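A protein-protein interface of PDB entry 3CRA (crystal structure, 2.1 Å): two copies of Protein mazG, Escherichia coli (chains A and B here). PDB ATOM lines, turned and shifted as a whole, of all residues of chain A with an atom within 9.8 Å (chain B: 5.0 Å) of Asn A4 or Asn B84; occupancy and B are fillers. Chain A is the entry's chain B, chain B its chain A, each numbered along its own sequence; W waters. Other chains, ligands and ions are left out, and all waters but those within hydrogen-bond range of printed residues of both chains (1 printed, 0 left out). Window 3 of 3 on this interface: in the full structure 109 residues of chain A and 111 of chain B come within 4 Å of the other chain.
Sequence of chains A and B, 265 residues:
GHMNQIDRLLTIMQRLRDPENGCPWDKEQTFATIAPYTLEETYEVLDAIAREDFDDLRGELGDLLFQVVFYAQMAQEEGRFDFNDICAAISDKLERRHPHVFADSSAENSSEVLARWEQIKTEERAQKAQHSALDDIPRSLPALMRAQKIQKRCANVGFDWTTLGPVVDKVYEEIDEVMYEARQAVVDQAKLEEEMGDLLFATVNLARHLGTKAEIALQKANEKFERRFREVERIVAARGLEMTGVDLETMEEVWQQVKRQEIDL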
ATOM      1  N   ASN A   4      15.189  19.043   3.390  1.00  0.00           N
ATOM      2  CA  ASN A   4      15.248  20.469   2.924  1.00  0.00           C
ATOM      3  C   ASN A   4      14.199  21.398   3.606  1.00  0.00           C
ATOM      4  O   ASN A   4      13.385  22.077   2.933  1.00  0.00           O
ATOM      5  CB  ASN A   4      15.113  20.523   1.400  1.00  0.00           C
ATOM      6  CG  ASN A   4      15.761  21.755   0.787  1.00  0.00           C
ATOM      7  OD1 ASN A   4      16.477  22.508   1.457  1.00  0.00           O
ATOM      8  ND2 ASN A   4      15.511  21.970  -0.504  1.00  0.00           N
ATOM      9  N   GLN A   5      14.232  21.424   4.946  1.00  0.00           N
ATOM     10  CA  GLN A   5      13.267  22.223   5.734  1.00  0.00           C
ATOM     11  C   GLN A   5      13.620  23.714   5.750  1.00  0.00           C
ATOM     12  O   GLN A   5      12.876  24.551   6.242  1.00  0.00           O
ATOM     13  CB  GLN A   5      13.156  21.675   7.149  1.00  0.00           C
ATOM     14  CG  GLN A   5      11.704  21.440   7.564  1.00  0.00           C
ATOM     15  CD  GLN A   5      11.281  20.007   7.383  1.00  0.00           C
ATOM     16  OE1 GLN A   5      10.758  19.390   8.317  1.00  0.00           O
ATOM     17  NE2 GLN A   5      11.494  19.458   6.186  1.00  0.00           N
ATOM     18  N   ILE A   6      14.777  24.007   5.169  1.00  0.00           N
ATOM     19  CA  ILE A   6      15.293  25.345   5.053  1.00  0.00           C
ATOM     20  C   ILE A   6      14.371  26.152   4.124  1.00  0.00           C
ATOM     21  O   ILE A   6      13.927  27.247   4.474  1.00  0.00           O
ATOM     22  CB  ILE A   6      16.741  25.323   4.522  1.00  0.00           C
ATOM     23  CG1 ILE A   6      17.611  24.294   5.301  1.00  0.00           C
ATOM     24  CG2 ILE A   6      17.342  26.757   4.606  1.00  0.00           C
ATOM     25  CD1 ILE A   6      17.423  22.728   5.040  1.00  0.00           C
ATOM     26  N   ASP A   7      14.059  25.563   2.968  1.00  0.00           N
ATOM     27  CA  ASP A   7      13.052  26.081   2.050  1.00  0.00           C
ATOM     28  C   ASP A   7      11.687  26.204   2.680  1.00  0.00           C
ATOM     29  O   ASP A   7      10.905  27.034   2.271  1.00  0.00           O
ATOM     30  CB  ASP A   7      12.909  25.170   0.824  1.00  0.00           C
ATOM     31  CG  ASP A   7      14.023  25.384  -0.195  1.00  0.00           C
ATOM     32  OD1 ASP A   7      14.923  26.235   0.066  1.00  0.00           O
ATOM     33  OD2 ASP A   7      13.987  24.701  -1.259  1.00  0.00           O
ATOM     34  N   ARG A   8      11.406  25.372   3.667  1.00  0.00           N
ATOM     35  CA  ARG A   8      10.077  25.340   4.224  1.00  0.00           C
ATOM     36  C   ARG A   8       9.910  26.437   5.234  1.00  0.00           C
ATOM     37  O   ARG A   8       8.789  26.936   5.399  1.00  0.00           O
ATOM     38  CB  ARG A   8       9.752  24.030   4.918  1.00  0.00           C
ATOM     39  CG  ARG A   8       8.544  24.238   5.849  1.00  0.00           C
ATOM     40  CD  ARG A   8       7.785  22.992   6.146  1.00  0.00           C
ATOM     41  NE  ARG A   8       8.364  22.239   7.244  1.00  0.00           N
ATOM     42  CZ  ARG A   8       7.720  21.963   8.365  1.00  0.00           C
ATOM     43  NH1 ARG A   8       6.479  22.392   8.516  1.00  0.00           N
ATOM     44  NH2 ARG A   8       8.322  21.247   9.323  1.00  0.00           N
ATOM     45  N   LEU A   9      10.999  26.738   5.968  1.00  0.00           N
ATOM     46  CA  LEU A   9      10.947  27.730   7.020  1.00  0.00           C
ATOM     47  C   LEU A   9      10.788  29.069   6.314  1.00  0.00           C
ATOM     48  O   LEU A   9       9.945  29.890   6.705  1.00  0.00           O
ATOM     49  CB  LEU A   9      12.245  27.728   7.829  1.00  0.00           C
ATOM     50  CG  LEU A   9      12.428  28.071   9.315  1.00  0.00           C
ATOM     51  CD1 LEU A   9      13.833  28.621   9.476  1.00  0.00           C
ATOM     52  CD2 LEU A   9      11.393  28.986   9.946  1.00  0.00           C
ATOM     53  N   LEU A  10      11.618  29.259   5.281  1.00  0.00           N
ATOM     54  CA  LEU A  10      11.582  30.444   4.470  1.00  0.00           C
ATOM     55  C   LEU A  10      10.160  30.724   4.047  1.00  0.00           C
ATOM     56  O   LEU A  10       9.630  31.774   4.395  1.00  0.00           O
ATOM     57  CB  LEU A  10      12.556  30.409   3.257  1.00  0.00           C
ATOM     58  CG  LEU A  10      14.097  30.462   3.501  1.00  0.00           C
ATOM     59  CD1 LEU A  10      14.886  30.256   2.203  1.00  0.00           C
ATOM     60  CD2 LEU A  10      14.623  31.740   4.262  1.00  0.00           C
ATOM     61  N   THR A  11       9.517  29.799   3.334  1.00  0.00           N
ATOM     62  CA  THR A  11       8.147  30.085   2.865  1.00  0.00           C
ATOM     63  C   THR A  11       7.164  30.284   4.054  1.00  0.00           C
ATOM     64  O   THR A  11       6.234  31.087   3.964  1.00  0.00           O
ATOM     65  CB  THR A  11       7.593  29.108   1.744  1.00  0.00           C
ATOM     66  OG1 THR A  11       6.940  28.007   2.355  1.00  0.00           O
ATOM     67  CG2 THR A  11       8.684  28.614   0.771  1.00  0.00           C
ATOM     68  N   ILE A  12       7.380  29.591   5.160  1.00  0.00           N
ATOM     69  CA  ILE A  12       6.645  29.906   6.390  1.00  0.00           C
ATOM     70  C   ILE A  12       6.824  31.385   6.842  1.00  0.00           C
ATOM     71  O   ILE A  12       5.926  31.948   7.459  1.00  0.00           O
ATOM     72  CB  ILE A  12       7.054  28.956   7.531  1.00  0.00           C
ATOM     73  CG1 ILE A  12       6.246  27.663   7.483  1.00  0.00           C
ATOM     74  CG2 ILE A  12       6.928  29.612   8.892  1.00  0.00           C
ATOM     75  CD1 ILE A  12       6.964  26.479   8.105  1.00  0.00           C
ATOM     76  N   ARG A  58      19.188  22.574  20.449  1.00  0.00           N
ATOM     77  CA  ARG A  58      18.559  22.448  19.120  1.00  0.00           C
ATOM     78  C   ARG A  58      17.401  23.411  18.936  1.00  0.00           C
ATOM     79  O   ARG A  58      17.226  24.002  17.837  1.00  0.00           O
ATOM     80  CB  ARG A  58      18.054  21.009  18.810  1.00  0.00           C
ATOM     81  CG  ARG A  58      17.554  20.882  17.313  1.00  0.00           C
ATOM     82  CD  ARG A  58      16.540  19.748  17.046  1.00  0.00           C
ATOM     83  NE  ARG A  58      16.898  18.513  17.721  1.00  0.00           N
ATOM     84  CZ  ARG A  58      16.408  18.080  18.890  1.00  0.00           C
ATOM     85  NH1 ARG A  58      15.507  18.790  19.574  1.00  0.00           N
ATOM     86  NH2 ARG A  58      16.847  16.927  19.387  1.00  0.00           N
ATOM     87  N   GLY A  62      16.956  27.055  16.695  1.00  0.00           N
ATOM     88  CA  GLY A  62      15.769  27.237  15.853  1.00  0.00           C
ATOM     89  C   GLY A  62      15.215  28.636  16.066  1.00  0.00           C
ATOM     90  O   GLY A  62      15.046  29.395  15.105  1.00  0.00           O
ATOM     91  N   LEU A  65      17.766  31.086  14.530  1.00  0.00           N
ATOM     92  CA  LEU A  65      17.656  30.959  13.062  1.00  0.00           C
ATOM     93  C   LEU A  65      16.450  31.694  12.500  1.00  0.00           C
ATOM     94  O   LEU A  65      16.508  32.315  11.416  1.00  0.00           O
ATOM     95  CB  LEU A  65      17.473  29.508  12.665  1.00  0.00           C
ATOM     96  CG  LEU A  65      17.932  29.095  11.257  1.00  0.00           C
ATOM     97  CD1 LEU A  65      17.148  27.851  10.647  1.00  0.00           C
ATOM     98  CD2 LEU A  65      18.106  30.189  10.276  1.00  0.00           C
ATOM     99  N   PHE A  83      17.726  36.524   1.902  1.00  0.00           N
ATOM    100  CA  PHE A  83      18.279  35.341   2.643  1.00  0.00           C
ATOM    101  C   PHE A  83      19.390  34.594   1.924  1.00  0.00           C
ATOM    102  O   PHE A  83      20.421  34.268   2.530  1.00  0.00           O
ATOM    103  CB  PHE A  83      17.264  34.313   3.145  1.00  0.00           C
ATOM    104  CG  PHE A  83      17.925  33.177   3.990  1.00  0.00           C
ATOM    105  CD1 PHE A  83      18.157  33.340   5.374  1.00  0.00           C
ATOM    106  CD2 PHE A  83      18.339  31.984   3.400  1.00  0.00           C
ATOM    107  CE1 PHE A  83      18.775  32.321   6.139  1.00  0.00           C
ATOM    108  CE2 PHE A  83      18.958  30.962   4.152  1.00  0.00           C
ATOM    109  CZ  PHE A  83      19.166  31.133   5.528  1.00  0.00           C
ATOM    110  N   ASN A  84      19.196  34.307   0.645  1.00  0.00           N
ATOM    111  CA  ASN A  84      20.318  33.748  -0.087  1.00  0.00           C
ATOM    112  C   ASN A  84      21.551  34.686  -0.310  1.00  0.00           C
ATOM    113  O   ASN A  84      22.669  34.212  -0.287  1.00  0.00           O
ATOM    114  CB  ASN A  84      19.846  32.989  -1.330  1.00  0.00           C
ATOM    115  CG  ASN A  84      19.905  31.492  -1.136  1.00  0.00           C
ATOM    116  OD1 ASN A  84      20.964  30.893  -1.325  1.00  0.00           O
ATOM    117  ND2 ASN A  84      18.770  30.871  -0.741  1.00  0.00           N
ATOM    118  N   ASP B  82      21.259  17.933  12.855  1.00  0.00           N
ATOM    119  CA  ASP B  82      21.793  18.705  11.746  1.00  0.00           C
ATOM    120  C   ASP B  82      20.963  19.955  11.509  1.00  0.00           C
ATOM    121  O   ASP B  82      19.944  20.173  12.169  1.00  0.00           O
ATOM    122  CB  ASP B  82      21.928  17.853  10.475  1.00  0.00           C
ATOM    123  CG  ASP B  82      20.589  17.366   9.881  1.00  0.00           C
ATOM    124  OD1 ASP B  82      20.661  16.482   8.973  1.00  0.00           O
ATOM    125  OD2 ASP B  82      19.481  17.811  10.244  1.00  0.00           O
ATOM    126  N   PHE B  83      21.434  20.782  10.575  1.00  0.00           N
ATOM    127  CA  PHE B  83      20.772  22.025  10.207  1.00  0.00           C
ATOM    128  C   PHE B  83      19.304  21.841   9.838  1.00  0.00           C
ATOM    129  O   PHE B  83      18.431  22.558  10.337  1.00  0.00           O
ATOM    130  CB  PHE B  83      21.536  22.705   9.067  1.00  0.00           C
ATOM    131  CG  PHE B  83      21.072  24.084   8.785  1.00  0.00           C
ATOM    132  CD1 PHE B  83      21.405  25.133   9.647  1.00  0.00           C
ATOM    133  CD2 PHE B  83      20.316  24.362   7.648  1.00  0.00           C
ATOM    134  CE1 PHE B  83      20.929  26.436   9.408  1.00  0.00           C
ATOM    135  CE2 PHE B  83      19.852  25.673   7.356  1.00  0.00           C
ATOM    136  CZ  PHE B  83      20.175  26.721   8.232  1.00  0.00           C
ATOM    137  N   ASN B  84      19.022  20.877   8.951  1.00  0.00           N
ATOM    138  CA  ASN B  84      17.633  20.524   8.562  1.00  0.00           C
ATOM    139  C   ASN B  84      16.727  20.194   9.762  1.00  0.00           C
ATOM    140  O   ASN B  84      15.554  20.649   9.810  1.00  0.00           O
ATOM    141  CB  ASN B  84      17.708  19.359   7.526  1.00  0.00           C
ATOM    142  CG  ASN B  84      16.327  18.873   7.040  1.00  0.00           C
ATOM    143  OD1 ASN B  84      15.559  19.633   6.418  1.00  0.00           O
ATOM    144  ND2 ASN B  84      16.016  17.580   7.309  1.00  0.00           N
ATOM    145  N   ASP B  85      17.236  19.425  10.741  1.00  0.00           N
ATOM    146  CA  ASP B  85      16.468  19.160  12.010  1.00  0.00           C
ATOM    147  C   ASP B  85      16.217  20.489  12.825  1.00  0.00           C
ATOM    148  O   ASP B  85      15.161  20.656  13.435  1.00  0.00           O
ATOM    149  CB  ASP B  85      17.186  18.235  12.994  1.00  0.00           C
ATOM    150  CG  ASP B  85      17.603  16.918  12.407  1.00  0.00           C
ATOM    151  OD1 ASP B  85      16.926  16.416  11.506  1.00  0.00           O
ATOM    152  OD2 ASP B  85      18.614  16.375  12.907  1.00  0.00           O
ATOM    153  N   ILE B  86      17.213  21.393  12.863  1.00  0.00           N
ATOM    154  CA  ILE B  86      16.963  22.734  13.450  1.00  0.00           C
ATOM    155  C   ILE B  86      15.830  23.391  12.653  1.00  0.00           C
ATOM    156  O   ILE B  86      14.835  23.833  13.226  1.00  0.00           O
ATOM    157  CB  ILE B  86      18.215  23.651  13.436  1.00  0.00           C
ATOM    158  CG1 ILE B  86      19.352  23.116  14.316  1.00  0.00           C
ATOM    159  CG2 ILE B  86      17.841  25.085  13.886  1.00  0.00           C
ATOM    160  CD1 ILE B  86      20.614  23.961  14.110  1.00  0.00           C
ATOM    161  N   CYS B  87      15.947  23.449  11.338  1.00  0.00           N
ATOM    162  CA  CYS B  87      14.908  24.145  10.576  1.00  0.00           C
ATOM    163  C   CYS B  87      13.590  23.413  10.687  1.00  0.00           C
ATOM    164  O   CYS B  87      12.539  24.051  10.768  1.00  0.00           O
ATOM    165  CB  CYS B  87      15.294  24.357   9.105  1.00  0.00           C
ATOM    166  SG  CYS B  87      16.896  25.101   8.790  1.00  0.00           S
ATOM    167  N   ALA B  88      13.638  22.076  10.721  1.00  0.00           N
ATOM    168  CA  ALA B  88      12.422  21.230  10.942  1.00  0.00           C
ATOM    169  C   ALA B  88      11.669  21.559  12.222  1.00  0.00           C
ATOM    170  O   ALA B  88      10.454  21.740  12.202  1.00  0.00           O
ATOM    171  CB  ALA B  88      12.774  19.688  10.907  1.00  0.00           C
ATOM    172  N   ALA B  89      12.376  21.599  13.345  1.00  0.00           N
ATOM    173  CA  ALA B  89      11.753  21.904  14.632  1.00  0.00           C
ATOM    174  C   ALA B  89      11.183  23.330  14.751  1.00  0.00           C
ATOM    175  O   ALA B  89      10.078  23.481  15.248  1.00  0.00           O
ATOM    176  CB  ALA B  89      12.716  21.614  15.767  1.00  0.00           C
HETATM  177  O   HOH W   1      15.075  24.264  15.913  1.00  0.00           O
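CB of Cys B87 touches O of Gln A5 (3.8 Å). Gln A5 touches Ala B88. Phe B83 touches Ile A6. CD1 of Ile A6 touches OD1 of Asn B84, at 3.9 Å. Ile A6 touches Cys B87 (CG1 to SG, 3.7 Å). Ala B88 touches Arg A8. Asp B85 touches Arg A58 (O to CD, 3.97 Å). Gly A62 touches Ile B86 (N to CG2, 3.5 Å). Leu A65 touches Cys B87 (CD1 to SG, 3.3 Å).
N of Asn B84 lies close to OD2 of Asp B82, 3.4 Å away. The side-chain carboxylate (OD2) of Asp B82 is in hydrogen-bond range of the backbone NH (N) of Asp B85, 2.8 Å away. O of Phe B83 lies close to SG of Cys B87 (3.3 Å). The side-chain carboxylate (OD2) of Asp A7 lies within hydrogen-bond range of the side-chain amide nitrogen (ND2) of Asn A4. The side-chain amide oxygen (OE1) of Gln A5 lies within hydrogen-bond range of the guanidinium group (NH2) of Arg A8 (3.2 Å).
The side-chain amide oxygen of Asn B84 lies within hydrogen-bond range of the backbone NH of Asn A4, 3.1 Å away. The backbone NH (N) of Gln A5 is in hydrogen-bond range of the side-chain amide oxygen (OD1) of Asn B84 (2.7 Å).
Of the 14 printed residues of chain A, 7 touch a printed residue of chain B. Hydrophobic or aromatic side chains of chain A within 4 Å of the printed part of chain B: Ile A6 and Leu A65. Among the printed residues, no Asp or Glu carboxylate lies within 4 Å of a Lys or Arg side-chain nitrogen of the other chain.
Positions printed for both chains: 83 and 84.
Water W1 lies within hydrogen-bond range of O of Ile B86 (2.7 Å), O of Arg A58 (2.9 Å) and N of Gly A62 (3.5 Å).
Of chain A, only Asn A4, Gln A5 and Ile A6 come within 4 Å of Asn B84. Asp B85 touches just one residue of chain A: Arg A58 (3.97 Å). Of chain A, only Gln A5 (3.8 Å), Ile A6 (3.7 Å) and Leu A65 (3.3 Å) come within 4 Å of Cys B87. Of chain A, only Gln A5 and Arg A8 come within 4 Å of Ala B88. Of the printed residues of chain B, Arg A8 touches Ala B88. Printed residues of chain A within 4 Å of Ile B86: Gly A62. Of the printed residues of chain B, Ile A6 touches Phe B83 (3.3 Å), Asn B84 (3.9 Å) and Cys B87 (3.7 Å). Of the printed residues of chain B, Arg A58 touches Asp B85 (3.97 Å). The nearest printed residue of chain B that does not touch Gln A5 is Ala B89 (5.7 Å).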
